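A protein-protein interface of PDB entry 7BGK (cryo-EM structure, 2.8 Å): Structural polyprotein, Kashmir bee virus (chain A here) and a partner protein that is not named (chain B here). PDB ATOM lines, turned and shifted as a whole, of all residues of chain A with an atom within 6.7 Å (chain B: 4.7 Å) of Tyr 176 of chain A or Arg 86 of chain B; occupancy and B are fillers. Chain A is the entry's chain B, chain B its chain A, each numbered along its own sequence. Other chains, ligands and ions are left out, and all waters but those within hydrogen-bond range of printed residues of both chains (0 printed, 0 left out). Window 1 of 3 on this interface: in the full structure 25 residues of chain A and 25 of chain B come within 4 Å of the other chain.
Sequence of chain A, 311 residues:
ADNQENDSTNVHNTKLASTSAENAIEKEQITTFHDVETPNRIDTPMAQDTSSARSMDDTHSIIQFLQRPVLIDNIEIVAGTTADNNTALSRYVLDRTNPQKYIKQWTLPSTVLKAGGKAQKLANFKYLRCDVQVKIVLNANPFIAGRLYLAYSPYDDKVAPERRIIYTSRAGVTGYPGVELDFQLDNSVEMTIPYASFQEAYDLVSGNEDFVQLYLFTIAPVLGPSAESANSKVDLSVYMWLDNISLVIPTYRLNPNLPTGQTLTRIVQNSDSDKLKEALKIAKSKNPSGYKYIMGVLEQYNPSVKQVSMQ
Of the printed residues of chain B, Tyr 176 of chain A touches Arg 86 (3.4 Å), Ile 194 (3.5 Å) and Gly 195 (3.2 Å).
Of the printed residues of chain B, Gly 172 of chain A touches Gly 195.
Of the printed residues of chain B, Tyr 152 of chain A touches Trp 192.
Tyr 85 of chain B touches none of the printed residues of chain A.
The nearest printed residue of chain B that does not touch Tyr 176 of chain A is Tyr 85 of chain B (7.2 Å).
The nearest residue of chain A that does not touch Arg 86 of chain B is Val 159 of chain A (4.1 Å).
Tyr 152 of chain A touches Trp 192 of chain B (CE2 to CH2, 3.3 Å).
Pro 154 of chain A touches Trp 192 of chain B.
OH of Tyr 155 of chain A touches CZ of Phe 87 of chain B (3.1 Å).
CG2 of Ile 156 of chain B touches CZ of Arg 163 of chain A (3.5 Å).
Gly 172 of chain A touches Gly 195 of chain B.
O of Gly 175 of chain A touches C of Ile 194 of chain B (3.4 Å).
Tyr 176 of chain A touches Ile 194 of chain B.
CD2 of Tyr 176 of chain A touches N of Gly 195 of chain B, 3.2 Å away.
N of Ile 194 of chain B is in hydrogen-bond range of O of Leu 84 of chain B, 2.6 Å away.
The backbone carbonyl oxygen (O) of Arg 86 of chain B is in hydrogen-bond range of the backbone NH (N) of Ile 156 of chain B (3.0 Å).
O of Tyr 176 of chain A is in hydrogen-bond range of OH of Tyr 149 of chain A, at 2.7 Å.
N of Tyr 152 of chain A lies within hydrogen-bond range of O of Pro 177 of chain A, 3.3 Å away.
OD1 of Asp 156 of chain A sits at hydrogen-bond distance from OG of Ser 153 of chain A (2.6 Å).
The side-chain hydroxyl (OH) of Tyr 176 of chain A is in hydrogen-bond range of the backbone carbonyl oxygen (O) of Arg 163 of chain A, 3.3 Å away.
The guanidinium group (NH2) of Arg 86 of chain B lies within hydrogen-bond range of the side-chain hydroxyl (OG) of Ser 153 of chain A.
The guanidinium group (NE) of Arg 86 of chain B is in hydrogen-bond range of the backbone carbonyl oxygen (O) of Pro 154 of chain A, 2.6 Å away.
OD1 of Asp 156 of chain A is in salt-bridge range of NH2 of Arg 86 of chain B (3.6 Å).
The guanidinium group (NH1) of Arg 86 of chain B sits at hydrogen-bond distance from the backbone carbonyl oxygen (O) of Arg 163 of chain A (2.6 Å).
The side-chain hydroxyl of Tyr 176 of chain A sits at hydrogen-bond distance from the guanidinium group of Arg 86 of chain B (3.4 Å).
O of Gly 175 of chain A sits at hydrogen-bond distance from N of Gly 195 of chain B.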
ATOM      1  N   TYR A 149      -1.978  17.259 -14.838  1.00  0.00           N
ATOM      2  CA  TYR A 149      -2.791  17.227 -13.628  1.00  0.00           C
ATOM      3  C   TYR A 149      -3.276  15.800 -13.421  1.00  0.00           C
ATOM      4  O   TYR A 149      -4.065  15.287 -14.219  1.00  0.00           O
ATOM      5  CB  TYR A 149      -3.968  18.192 -13.718  1.00  0.00           C
ATOM      6  CG  TYR A 149      -4.666  18.432 -12.400  1.00  0.00           C
ATOM      7  CD1 TYR A 149      -4.039  19.129 -11.382  1.00  0.00           C
ATOM      8  CD2 TYR A 149      -5.946  17.966 -12.172  1.00  0.00           C
ATOM      9  CE1 TYR A 149      -4.666  19.351 -10.182  1.00  0.00           C
ATOM     10  CE2 TYR A 149      -6.576  18.184 -10.974  1.00  0.00           C
ATOM     11  CZ  TYR A 149      -5.931  18.877  -9.981  1.00  0.00           C
ATOM     12  OH  TYR A 149      -6.552  19.106  -8.779  1.00  0.00           O
ATOM     13  N   LEU A 150      -2.798  15.160 -12.364  1.00  0.00           N
ATOM     14  CA  LEU A 150      -3.267  13.840 -11.980  1.00  0.00           C
ATOM     15  C   LEU A 150      -4.410  13.995 -10.988  1.00  0.00           C
ATOM     16  O   LEU A 150      -4.223  14.548  -9.902  1.00  0.00           O
ATOM     17  CB  LEU A 150      -2.131  13.017 -11.380  1.00  0.00           C
ATOM     18  CG  LEU A 150      -2.466  11.600 -10.933  1.00  0.00           C
ATOM     19  CD1 LEU A 150      -2.526  10.681 -12.111  1.00  0.00           C
ATOM     20  CD2 LEU A 150      -1.442  11.118  -9.941  1.00  0.00           C
ATOM     21  N   ALA A 151      -5.588  13.513 -11.365  1.00  0.00           N
ATOM     22  CA  ALA A 151      -6.774  13.608 -10.534  1.00  0.00           C
ATOM     23  C   ALA A 151      -7.501  12.275 -10.546  1.00  0.00           C
ATOM     24  O   ALA A 151      -7.377  11.486 -11.484  1.00  0.00           O
ATOM     25  CB  ALA A 151      -7.706  14.716 -11.016  1.00  0.00           C
ATOM     26  N   TYR A 152      -8.263  12.030  -9.486  1.00  0.00           N
ATOM     27  CA  TYR A 152      -9.097  10.844  -9.377  1.00  0.00           C
ATOM     28  C   TYR A 152     -10.548  11.240  -9.166  1.00  0.00           C
ATOM     29  O   TYR A 152     -10.850  12.172  -8.416  1.00  0.00           O
ATOM     30  CB  TYR A 152      -8.617   9.914  -8.255  1.00  0.00           C
ATOM     31  CG  TYR A 152      -8.575  10.506  -6.870  1.00  0.00           C
ATOM     32  CD1 TYR A 152      -7.437  11.140  -6.407  1.00  0.00           C
ATOM     33  CD2 TYR A 152      -9.645  10.384  -6.007  1.00  0.00           C
ATOM     34  CE1 TYR A 152      -7.383  11.657  -5.142  1.00  0.00           C
ATOM     35  CE2 TYR A 152      -9.591  10.901  -4.747  1.00  0.00           C
ATOM     36  CZ  TYR A 152      -8.465  11.536  -4.317  1.00  0.00           C
ATOM     37  OH  TYR A 152      -8.431  12.049  -3.044  1.00  0.00           O
ATOM     38  N   SER A 153     -11.436  10.532  -9.858  1.00  0.00           N
ATOM     39  CA  SER A 153     -12.870  10.762  -9.800  1.00  0.00           C
ATOM     40  C   SER A 153     -13.564   9.513  -9.280  1.00  0.00           C
ATOM     41  O   SER A 153     -13.515   8.466  -9.945  1.00  0.00           O
ATOM     42  CB  SER A 153     -13.420  11.119 -11.174  1.00  0.00           C
ATOM     43  OG  SER A 153     -14.799  11.418 -11.100  1.00  0.00           O
ATOM     44  N   PRO A 154     -14.205   9.554  -8.116  1.00  0.00           N
ATOM     45  CA  PRO A 154     -14.907   8.364  -7.637  1.00  0.00           C
ATOM     46  C   PRO A 154     -16.200   8.135  -8.397  1.00  0.00           C
ATOM     47  O   PRO A 154     -16.929   9.075  -8.722  1.00  0.00           O
ATOM     48  CB  PRO A 154     -15.165   8.672  -6.159  1.00  0.00           C
ATOM     49  CG  PRO A 154     -14.322   9.822  -5.844  1.00  0.00           C
ATOM     50  CD  PRO A 154     -14.112  10.583  -7.073  1.00  0.00           C
ATOM     51  N   TYR A 155     -16.484   6.865  -8.668  1.00  0.00           N
ATOM     52  CA  TYR A 155     -17.732   6.452  -9.303  1.00  0.00           C
ATOM     53  C   TYR A 155     -17.943   7.139 -10.644  1.00  0.00           C
ATOM     54  O   TYR A 155     -19.075   7.290 -11.103  1.00  0.00           O
ATOM     55  CB  TYR A 155     -18.921   6.709  -8.379  1.00  0.00           C
ATOM     56  CG  TYR A 155     -18.776   6.035  -7.044  1.00  0.00           C
ATOM     57  CD1 TYR A 155     -19.171   4.725  -6.866  1.00  0.00           C
ATOM     58  CD2 TYR A 155     -18.219   6.700  -5.968  1.00  0.00           C
ATOM     59  CE1 TYR A 155     -19.028   4.104  -5.658  1.00  0.00           C
ATOM     60  CE2 TYR A 155     -18.073   6.085  -4.757  1.00  0.00           C
ATOM     61  CZ  TYR A 155     -18.480   4.787  -4.607  1.00  0.00           C
ATOM     62  OH  TYR A 155     -18.334   4.169  -3.396  1.00  0.00           O
ATOM     63  N   ASP A 156     -16.850   7.550 -11.286  1.00  0.00           N
ATOM     64  CA  ASP A 156     -16.956   8.282 -12.543  1.00  0.00           C
ATOM     65  C   ASP A 156     -17.657   7.451 -13.609  1.00  0.00           C
ATOM     66  O   ASP A 156     -18.398   7.989 -14.438  1.00  0.00           O
ATOM     67  CB  ASP A 156     -15.567   8.698 -13.015  1.00  0.00           C
ATOM     68  CG  ASP A 156     -15.599   9.903 -13.926  1.00  0.00           C
ATOM     69  OD1 ASP A 156     -15.826  11.019 -13.418  1.00  0.00           O
ATOM     70  OD2 ASP A 156     -15.392   9.737 -15.145  1.00  0.00           O
ATOM     71  N   VAL A 159     -21.504   7.133 -12.097  1.00  0.00           N
ATOM     72  CA  VAL A 159     -22.237   8.345 -11.761  1.00  0.00           C
ATOM     73  C   VAL A 159     -22.748   8.980 -13.044  1.00  0.00           C
ATOM     74  O   VAL A 159     -22.184   8.789 -14.126  1.00  0.00           O
ATOM     75  CB  VAL A 159     -21.348   9.317 -10.952  1.00  0.00           C
ATOM     76  CG1 VAL A 159     -20.267   9.923 -11.818  1.00  0.00           C
ATOM     77  CG2 VAL A 159     -22.174  10.382 -10.283  1.00  0.00           C
ATOM     78  N   ALA A 160     -23.838   9.731 -12.924  1.00  0.00           N
ATOM     79  CA  ALA A 160     -24.463  10.393 -14.059  1.00  0.00           C
ATOM     80  C   ALA A 160     -23.427  11.183 -14.846  1.00  0.00           C
ATOM     81  O   ALA A 160     -22.424  11.628 -14.276  1.00  0.00           O
ATOM     82  CB  ALA A 160     -25.585  11.312 -13.588  1.00  0.00           C
ATOM     83  N   GLU A 162     -23.302  14.250 -16.178  1.00  0.00           N
ATOM     84  CA  GLU A 162     -23.062  15.617 -15.735  1.00  0.00           C
ATOM     85  C   GLU A 162     -22.166  15.677 -14.509  1.00  0.00           C
ATOM     86  O   GLU A 162     -21.559  16.722 -14.251  1.00  0.00           O
ATOM     87  CB  GLU A 162     -24.391  16.309 -15.444  1.00  0.00           C
ATOM     88  CG  GLU A 162     -25.300  15.559 -14.488  1.00  0.00           C
ATOM     89  CD  GLU A 162     -26.343  14.716 -15.191  1.00  0.00           C
ATOM     90  OE1 GLU A 162     -26.173  14.425 -16.393  1.00  0.00           O
ATOM     91  OE2 GLU A 162     -27.335  14.342 -14.536  1.00  0.00           O
ATOM     92  N   ARG A 163     -22.058  14.585 -13.758  1.00  0.00           N
ATOM     93  CA  ARG A 163     -21.283  14.543 -12.530  1.00  0.00           C
ATOM     94  C   ARG A 163     -19.888  13.969 -12.732  1.00  0.00           C
ATOM     95  O   ARG A 163     -19.175  13.749 -11.749  1.00  0.00           O
ATOM     96  CB  ARG A 163     -22.026  13.726 -11.479  1.00  0.00           C
ATOM     97  CG  ARG A 163     -23.373  14.273 -11.099  1.00  0.00           C
ATOM     98  CD  ARG A 163     -24.112  13.317 -10.212  1.00  0.00           C
ATOM     99  NE  ARG A 163     -25.389  13.847  -9.750  1.00  0.00           N
ATOM    100  CZ  ARG A 163     -25.538  14.618  -8.681  1.00  0.00           C
ATOM    101  NH1 ARG A 163     -24.494  14.959  -7.952  1.00  0.00           N
ATOM    102  NH2 ARG A 163     -26.738  15.050  -8.340  1.00  0.00           N
ATOM    103  N   ARG A 164     -19.484  13.728 -13.972  1.00  0.00           N
ATOM    104  CA  ARG A 164     -18.216  13.081 -14.263  1.00  0.00           C
ATOM    105  C   ARG A 164     -17.115  14.108 -14.490  1.00  0.00           C
ATOM    106  O   ARG A 164     -17.358  15.216 -14.969  1.00  0.00           O
ATOM    107  CB  ARG A 164     -18.349  12.186 -15.491  1.00  0.00           C
ATOM    108  CG  ARG A 164     -19.232  10.980 -15.285  1.00  0.00           C
ATOM    109  CD  ARG A 164     -19.340  10.166 -16.546  1.00  0.00           C
ATOM    110  NE  ARG A 164     -18.068   9.553 -16.905  1.00  0.00           N
ATOM    111  CZ  ARG A 164     -17.948   8.442 -17.623  1.00  0.00           C
ATOM    112  NH1 ARG A 164     -19.024   7.816 -18.078  1.00  0.00           N
ATOM    113  NH2 ARG A 164     -16.746   7.960 -17.892  1.00  0.00           N
ATOM    114  N   ILE A 165     -15.889  13.723 -14.128  1.00  0.00           N
ATOM    115  CA  ILE A 165     -14.730  14.567 -14.396  1.00  0.00           C
ATOM    116  C   ILE A 165     -14.550  14.738 -15.895  1.00  0.00           C
ATOM    117  O   ILE A 165     -14.157  15.806 -16.376  1.00  0.00           O
ATOM    118  CB  ILE A 165     -13.480  13.976 -13.722  1.00  0.00           C
ATOM    119  CG1 ILE A 165     -12.338  14.983 -13.744  1.00  0.00           C
ATOM    120  CG2 ILE A 165     -13.072  12.701 -14.388  1.00  0.00           C
ATOM    121  CD1 ILE A 165     -11.189  14.611 -12.883  1.00  0.00           C
ATOM    122  N   ILE A 166     -14.799  13.675 -16.652  1.00  0.00           N
ATOM    123  CA  ILE A 166     -15.104  13.822 -18.063  1.00  0.00           C
ATOM    124  C   ILE A 166     -16.470  14.478 -18.169  1.00  0.00           C
ATOM    125  O   ILE A 166     -17.360  14.234 -17.343  1.00  0.00           O
ATOM    126  CB  ILE A 166     -15.069  12.451 -18.761  1.00  0.00           C
ATOM    127  CG1 ILE A 166     -13.753  11.730 -18.482  1.00  0.00           C
ATOM    128  CG2 ILE A 166     -15.251  12.588 -20.241  1.00  0.00           C
ATOM    129  CD1 ILE A 166     -12.524  12.503 -18.848  1.00  0.00           C
ATOM    130  N   THR A 168     -16.924  17.774 -17.879  1.00  0.00           N
ATOM    131  CA  THR A 168     -16.930  19.020 -17.127  1.00  0.00           C
ATOM    132  C   THR A 168     -15.787  19.898 -17.611  1.00  0.00           C
ATOM    133  O   THR A 168     -15.017  19.528 -18.501  1.00  0.00           O
ATOM    134  CB  THR A 168     -16.843  18.797 -15.611  1.00  0.00           C
ATOM    135  OG1 THR A 168     -17.207  20.008 -14.944  1.00  0.00           O
ATOM    136  CG2 THR A 168     -15.456  18.411 -15.179  1.00  0.00           C
ATOM    137  N   ALA A 171     -11.928  24.197 -15.048  1.00  0.00           N
ATOM    138  CA  ALA A 171     -12.038  24.629 -13.666  1.00  0.00           C
ATOM    139  C   ALA A 171     -12.760  23.606 -12.807  1.00  0.00           C
ATOM    140  O   ALA A 171     -12.603  23.619 -11.583  1.00  0.00           O
ATOM    141  CB  ALA A 171     -12.759  25.971 -13.597  1.00  0.00           C
ATOM    142  N   GLY A 172     -13.549  22.731 -13.418  1.00  0.00           N
ATOM    143  CA  GLY A 172     -14.171  21.640 -12.706  1.00  0.00           C
ATOM    144  C   GLY A 172     -13.218  20.485 -12.519  1.00  0.00           C
ATOM    145  O   GLY A 172     -13.108  19.927 -11.427  1.00  0.00           O
ATOM    146  N   VAL A 173     -12.521  20.115 -13.591  1.00  0.00           N
ATOM    147  CA  VAL A 173     -11.511  19.068 -13.498  1.00  0.00           C
ATOM    148  C   VAL A 173     -10.494  19.414 -12.421  1.00  0.00           C
ATOM    149  O   VAL A 173     -10.213  18.611 -11.526  1.00  0.00           O
ATOM    150  CB  VAL A 173     -10.839  18.853 -14.864  1.00  0.00           C
ATOM    151  CG1 VAL A 173      -9.659  17.944 -14.736  1.00  0.00           C
ATOM    152  CG2 VAL A 173     -11.813  18.267 -15.837  1.00  0.00           C
ATOM    153  N   THR A 174      -9.926  20.612 -12.492  1.00  0.00           N
ATOM    154  CA  THR A 174      -8.925  21.027 -11.522  1.00  0.00           C
ATOM    155  C   THR A 174      -9.510  21.322 -10.153  1.00  0.00           C
ATOM    156  O   THR A 174      -8.752  21.638  -9.232  1.00  0.00           O
ATOM    157  CB  THR A 174      -8.190  22.246 -12.050  1.00  0.00           C
ATOM    158  OG1 THR A 174      -9.133  23.274 -12.364  1.00  0.00           O
ATOM    159  CG2 THR A 174      -7.430  21.877 -13.289  1.00  0.00           C
ATOM    160  N   GLY A 175     -10.825  21.228  -9.998  1.00  0.00           N
ATOM    161  CA  GLY A 175     -11.432  21.241  -8.688  1.00  0.00           C
ATOM    162  C   GLY A 175     -11.475  19.895  -8.018  1.00  0.00           C
ATOM    163  O   GLY A 175     -11.851  19.805  -6.847  1.00  0.00           O
ATOM    164  N   TYR A 176     -11.099  18.849  -8.736  1.00  0.00           N
ATOM    165  CA  TYR A 176     -11.027  17.516  -8.184  1.00  0.00           C
ATOM    166  C   TYR A 176      -9.729  17.329  -7.412  1.00  0.00           C
ATOM    167  O   TYR A 176      -8.763  18.070  -7.606  1.00  0.00           O
ATOM    168  CB  TYR A 176     -11.119  16.484  -9.300  1.00  0.00           C
ATOM    169  CG  TYR A 176     -12.525  16.127  -9.713  1.00  0.00           C
ATOM    170  CD1 TYR A 176     -13.065  14.898  -9.395  1.00  0.00           C
ATOM    171  CD2 TYR A 176     -13.306  17.014 -10.427  1.00  0.00           C
ATOM    172  CE1 TYR A 176     -14.342  14.566  -9.769  1.00  0.00           C
ATOM    173  CE2 TYR A 176     -14.584  16.687 -10.804  1.00  0.00           C
ATOM    174  CZ  TYR A 176     -15.096  15.467 -10.471  1.00  0.00           C
ATOM    175  OH  TYR A 176     -16.372  15.155 -10.852  1.00  0.00           O
ATOM    176  N   PRO A 177      -9.681  16.338  -6.524  1.00  0.00           N
ATOM    177  CA  PRO A 177      -8.440  16.058  -5.792  1.00  0.00           C
ATOM    178  C   PRO A 177      -7.358  15.561  -6.737  1.00  0.00           C
ATOM    179  O   PRO A 177      -7.506  14.521  -7.378  1.00  0.00           O
ATOM    180  CB  PRO A 177      -8.855  14.984  -4.785  1.00  0.00           C
ATOM    181  CG  PRO A 177     -10.118  14.440  -5.288  1.00  0.00           C
ATOM    182  CD  PRO A 177     -10.785  15.473  -6.086  1.00  0.00           C
ATOM    183  N   GLY A 178      -6.265  16.311  -6.816  1.00  0.00           N
ATOM    184  CA  GLY A 178      -5.197  15.949  -7.720  1.00  0.00           C
ATOM    185  C   GLY A 178      -3.900  16.645  -7.382  1.00  0.00           C
ATOM    186  O   GLY A 178      -3.809  17.421  -6.430  1.00  0.00           O
ATOM    187  N   VAL A 179      -2.893  16.354  -8.197  1.00  0.00           N
ATOM    188  CA  VAL A 179      -1.549  16.881  -8.030  1.00  0.00           C
ATOM    189  C   VAL A 179      -1.136  17.567  -9.320  1.00  0.00           C
ATOM    190  O   VAL A 179      -1.269  16.995 -10.405  1.00  0.00           O
ATOM    191  CB  VAL A 179      -0.538  15.777  -7.669  1.00  0.00           C
ATOM    192  CG1 VAL A 179       0.837  16.364  -7.513  1.00  0.00           C
ATOM    193  CG2 VAL A 179      -0.919  15.093  -6.411  1.00  0.00           C
ATOM    194  N   LEU B  84     -20.822  18.789  -5.807  1.00  0.00           N
ATOM    195  CA  LEU B  84     -19.505  18.971  -5.225  1.00  0.00           C
ATOM    196  C   LEU B  84     -19.009  17.743  -4.482  1.00  0.00           C
ATOM    197  O   LEU B  84     -17.842  17.713  -4.084  1.00  0.00           O
ATOM    198  CB  LEU B  84     -19.516  20.152  -4.254  1.00  0.00           C
ATOM    199  CG  LEU B  84     -19.722  21.550  -4.804  1.00  0.00           C
ATOM    200  CD1 LEU B  84     -20.020  22.477  -3.663  1.00  0.00           C
ATOM    201  CD2 LEU B  84     -18.503  22.007  -5.547  1.00  0.00           C
ATOM    202  N   TYR B  85     -19.858  16.738  -4.289  1.00  0.00           N
ATOM    203  CA  TYR B  85     -19.543  15.604  -3.441  1.00  0.00           C
ATOM    204  C   TYR B  85     -19.963  14.320  -4.138  1.00  0.00           C
ATOM    205  O   TYR B  85     -20.651  14.334  -5.160  1.00  0.00           O
ATOM    206  CB  TYR B  85     -20.229  15.729  -2.075  1.00  0.00           C
ATOM    207  CG  TYR B  85     -19.945  17.037  -1.377  1.00  0.00           C
ATOM    208  CD1 TYR B  85     -18.800  17.215  -0.623  1.00  0.00           C
ATOM    209  CD2 TYR B  85     -20.819  18.099  -1.483  1.00  0.00           C
ATOM    210  CE1 TYR B  85     -18.539  18.401  -0.004  1.00  0.00           C
ATOM    211  CE2 TYR B  85     -20.565  19.291  -0.863  1.00  0.00           C
ATOM    212  CZ  TYR B  85     -19.424  19.439  -0.125  1.00  0.00           C
ATOM    213  OH  TYR B  85     -19.170  20.634   0.495  1.00  0.00           O
ATOM    214  N   ARG B  86     -19.535  13.203  -3.563  1.00  0.00           N
ATOM    215  CA  ARG B  86     -19.804  11.875  -4.090  1.00  0.00           C
ATOM    216  C   ARG B  86     -20.629  11.007  -3.159  1.00  0.00           C
ATOM    217  O   ARG B  86     -21.376  10.155  -3.637  1.00  0.00           O
ATOM    218  CB  ARG B  86     -18.489  11.145  -4.390  1.00  0.00           C
ATOM    219  CG  ARG B  86     -17.729  11.660  -5.583  1.00  0.00           C
ATOM    220  CD  ARG B  86     -18.555  11.619  -6.842  1.00  0.00           C
ATOM    221  NE  ARG B  86     -17.733  11.462  -8.033  1.00  0.00           N
ATOM    222  CZ  ARG B  86     -17.860  12.176  -9.144  1.00  0.00           C
ATOM    223  NH1 ARG B  86     -18.776  13.123  -9.247  1.00  0.00           N
ATOM    224  NH2 ARG B  86     -17.057  11.942 -10.164  1.00  0.00           N
ATOM    225  N   PHE B  87     -20.508  11.197  -1.851  1.00  0.00           N
ATOM    226  CA  PHE B  87     -21.215  10.415  -0.852  1.00  0.00           C
ATOM    227  C   PHE B  87     -22.211  11.289  -0.108  1.00  0.00           C
ATOM    228  O   PHE B  87     -22.114  12.518  -0.101  1.00  0.00           O
ATOM    229  CB  PHE B  87     -20.238   9.791   0.147  1.00  0.00           C
ATOM    230  CG  PHE B  87     -19.452   8.643  -0.396  1.00  0.00           C
ATOM    231  CD1 PHE B  87     -20.069   7.634  -1.095  1.00  0.00           C
ATOM    232  CD2 PHE B  87     -18.093   8.568  -0.191  1.00  0.00           C
ATOM    233  CE1 PHE B  87     -19.354   6.584  -1.582  1.00  0.00           C
ATOM    234  CE2 PHE B  87     -17.371   7.509  -0.682  1.00  0.00           C
ATOM    235  CZ  PHE B  87     -18.006   6.521  -1.379  1.00  0.00           C
ATOM    236  N   TYR B  88     -23.179  10.634   0.525  1.00  0.00           N
ATOM    237  CA  TYR B  88     -24.069  11.308   1.454  1.00  0.00           C
ATOM    238  C   TYR B  88     -24.510  10.325   2.525  1.00  0.00           C
ATOM    239  O   TYR B  88     -24.391   9.108   2.372  1.00  0.00           O
ATOM    240  CB  TYR B  88     -25.278  11.928   0.745  1.00  0.00           C
ATOM    241  CG  TYR B  88     -26.361  10.969   0.317  1.00  0.00           C
ATOM    242  CD1 TYR B  88     -26.477  10.568  -1.002  1.00  0.00           C
ATOM    243  CD2 TYR B  88     -27.299  10.509   1.221  1.00  0.00           C
ATOM    244  CE1 TYR B  88     -27.475   9.713  -1.395  1.00  0.00           C
ATOM    245  CE2 TYR B  88     -28.297   9.656   0.839  1.00  0.00           C
ATOM    246  CZ  TYR B  88     -28.381   9.259  -0.471  1.00  0.00           C
ATOM    247  OH  TYR B  88     -29.379   8.407  -0.864  1.00  0.00           O
ATOM    248  N   ILE B 154     -23.951   6.612   1.346  1.00  0.00           N
ATOM    249  CA  ILE B 154     -24.673   6.292   0.120  1.00  0.00           C
ATOM    250  C   ILE B 154     -24.039   7.079  -1.017  1.00  0.00           C
ATOM    251  O   ILE B 154     -23.851   8.292  -0.882  1.00  0.00           O
ATOM    252  CB  ILE B 154     -26.172   6.621   0.233  1.00  0.00           C
ATOM    253  CG1 ILE B 154     -26.806   5.894   1.415  1.00  0.00           C
ATOM    254  CG2 ILE B 154     -26.886   6.269  -1.040  1.00  0.00           C
ATOM    255  CD1 ILE B 154     -26.699   4.402   1.366  1.00  0.00           C
ATOM    256  N   PRO B 155     -23.690   6.445  -2.132  1.00  0.00           N
ATOM    257  CA  PRO B 155     -23.139   7.203  -3.252  1.00  0.00           C
ATOM    258  C   PRO B 155     -24.239   7.797  -4.111  1.00  0.00           C
ATOM    259  O   PRO B 155     -25.290   7.188  -4.328  1.00  0.00           O
ATOM    260  CB  PRO B 155     -22.337   6.149  -4.017  1.00  0.00           C
ATOM    261  CG  PRO B 155     -23.060   4.917  -3.780  1.00  0.00           C
ATOM    262  CD  PRO B 155     -23.662   4.999  -2.408  1.00  0.00           C
ATOM    263  N   ILE B 156     -23.985   9.007  -4.595  1.00  0.00           N
ATOM    264  CA  ILE B 156     -24.882   9.677  -5.527  1.00  0.00           C
ATOM    265  C   ILE B 156     -24.850   8.978  -6.882  1.00  0.00           C
ATOM    266  O   ILE B 156     -25.601   9.334  -7.796  1.00  0.00           O
ATOM    267  CB  ILE B 156     -24.514  11.168  -5.640  1.00  0.00           C
ATOM    268  CG1 ILE B 156     -24.538  11.823  -4.260  1.00  0.00           C
ATOM    269  CG2 ILE B 156     -25.478  11.893  -6.524  1.00  0.00           C
ATOM    270  CD1 ILE B 156     -23.767  13.077  -4.169  1.00  0.00           C
ATOM    271  N   TRP B 192     -17.349  13.701   0.338  1.00  0.00           N
ATOM    272  CA  TRP B 192     -16.055  14.347   0.249  1.00  0.00           C
ATOM    273  C   TRP B 192     -15.870  14.986  -1.120  1.00  0.00           C
ATOM    274  O   TRP B 192     -16.352  14.484  -2.138  1.00  0.00           O
ATOM    275  CB  TRP B 192     -14.958  13.348   0.616  1.00  0.00           C
ATOM    276  CG  TRP B 192     -14.881  12.108  -0.201  1.00  0.00           C
ATOM    277  CD1 TRP B 192     -15.613  10.973  -0.025  1.00  0.00           C
ATOM    278  CD2 TRP B 192     -13.955  11.827  -1.250  1.00  0.00           C
ATOM    279  NE1 TRP B 192     -15.225  10.015  -0.923  1.00  0.00           N
ATOM    280  CE2 TRP B 192     -14.211  10.518  -1.689  1.00  0.00           C
ATOM    281  CE3 TRP B 192     -12.952  12.562  -1.876  1.00  0.00           C
ATOM    282  CZ2 TRP B 192     -13.506   9.933  -2.714  1.00  0.00           C
ATOM    283  CZ3 TRP B 192     -12.258  11.983  -2.896  1.00  0.00           C
ATOM    284  CH2 TRP B 192     -12.531  10.677  -3.304  1.00  0.00           C
ATOM    285  N   ILE B 194     -15.284  17.261  -4.501  1.00  0.00           N
ATOM    286  CA  ILE B 194     -14.782  17.098  -5.856  1.00  0.00           C
ATOM    287  C   ILE B 194     -14.987  18.411  -6.595  1.00  0.00           C
ATOM    288  O   ILE B 194     -15.385  19.418  -6.002  1.00  0.00           O
ATOM    289  CB  ILE B 194     -15.476  15.939  -6.592  1.00  0.00           C
ATOM    290  CG1 ILE B 194     -16.984  16.139  -6.588  1.00  0.00           C
ATOM    291  CG2 ILE B 194     -15.111  14.621  -5.965  1.00  0.00           C
ATOM    292  CD1 ILE B 194     -17.683  15.317  -7.559  1.00  0.00           C
ATOM    293  N   GLY B 195     -14.710  18.408  -7.885  1.00  0.00           N
ATOM    294  CA  GLY B 195     -14.836  19.600  -8.688  1.00  0.00           C
ATOM    295  C   GLY B 195     -16.257  19.912  -9.084  1.00  0.00           C
ATOM    296  O   GLY B 195     -17.175  19.106  -8.944  1.00  0.00           O
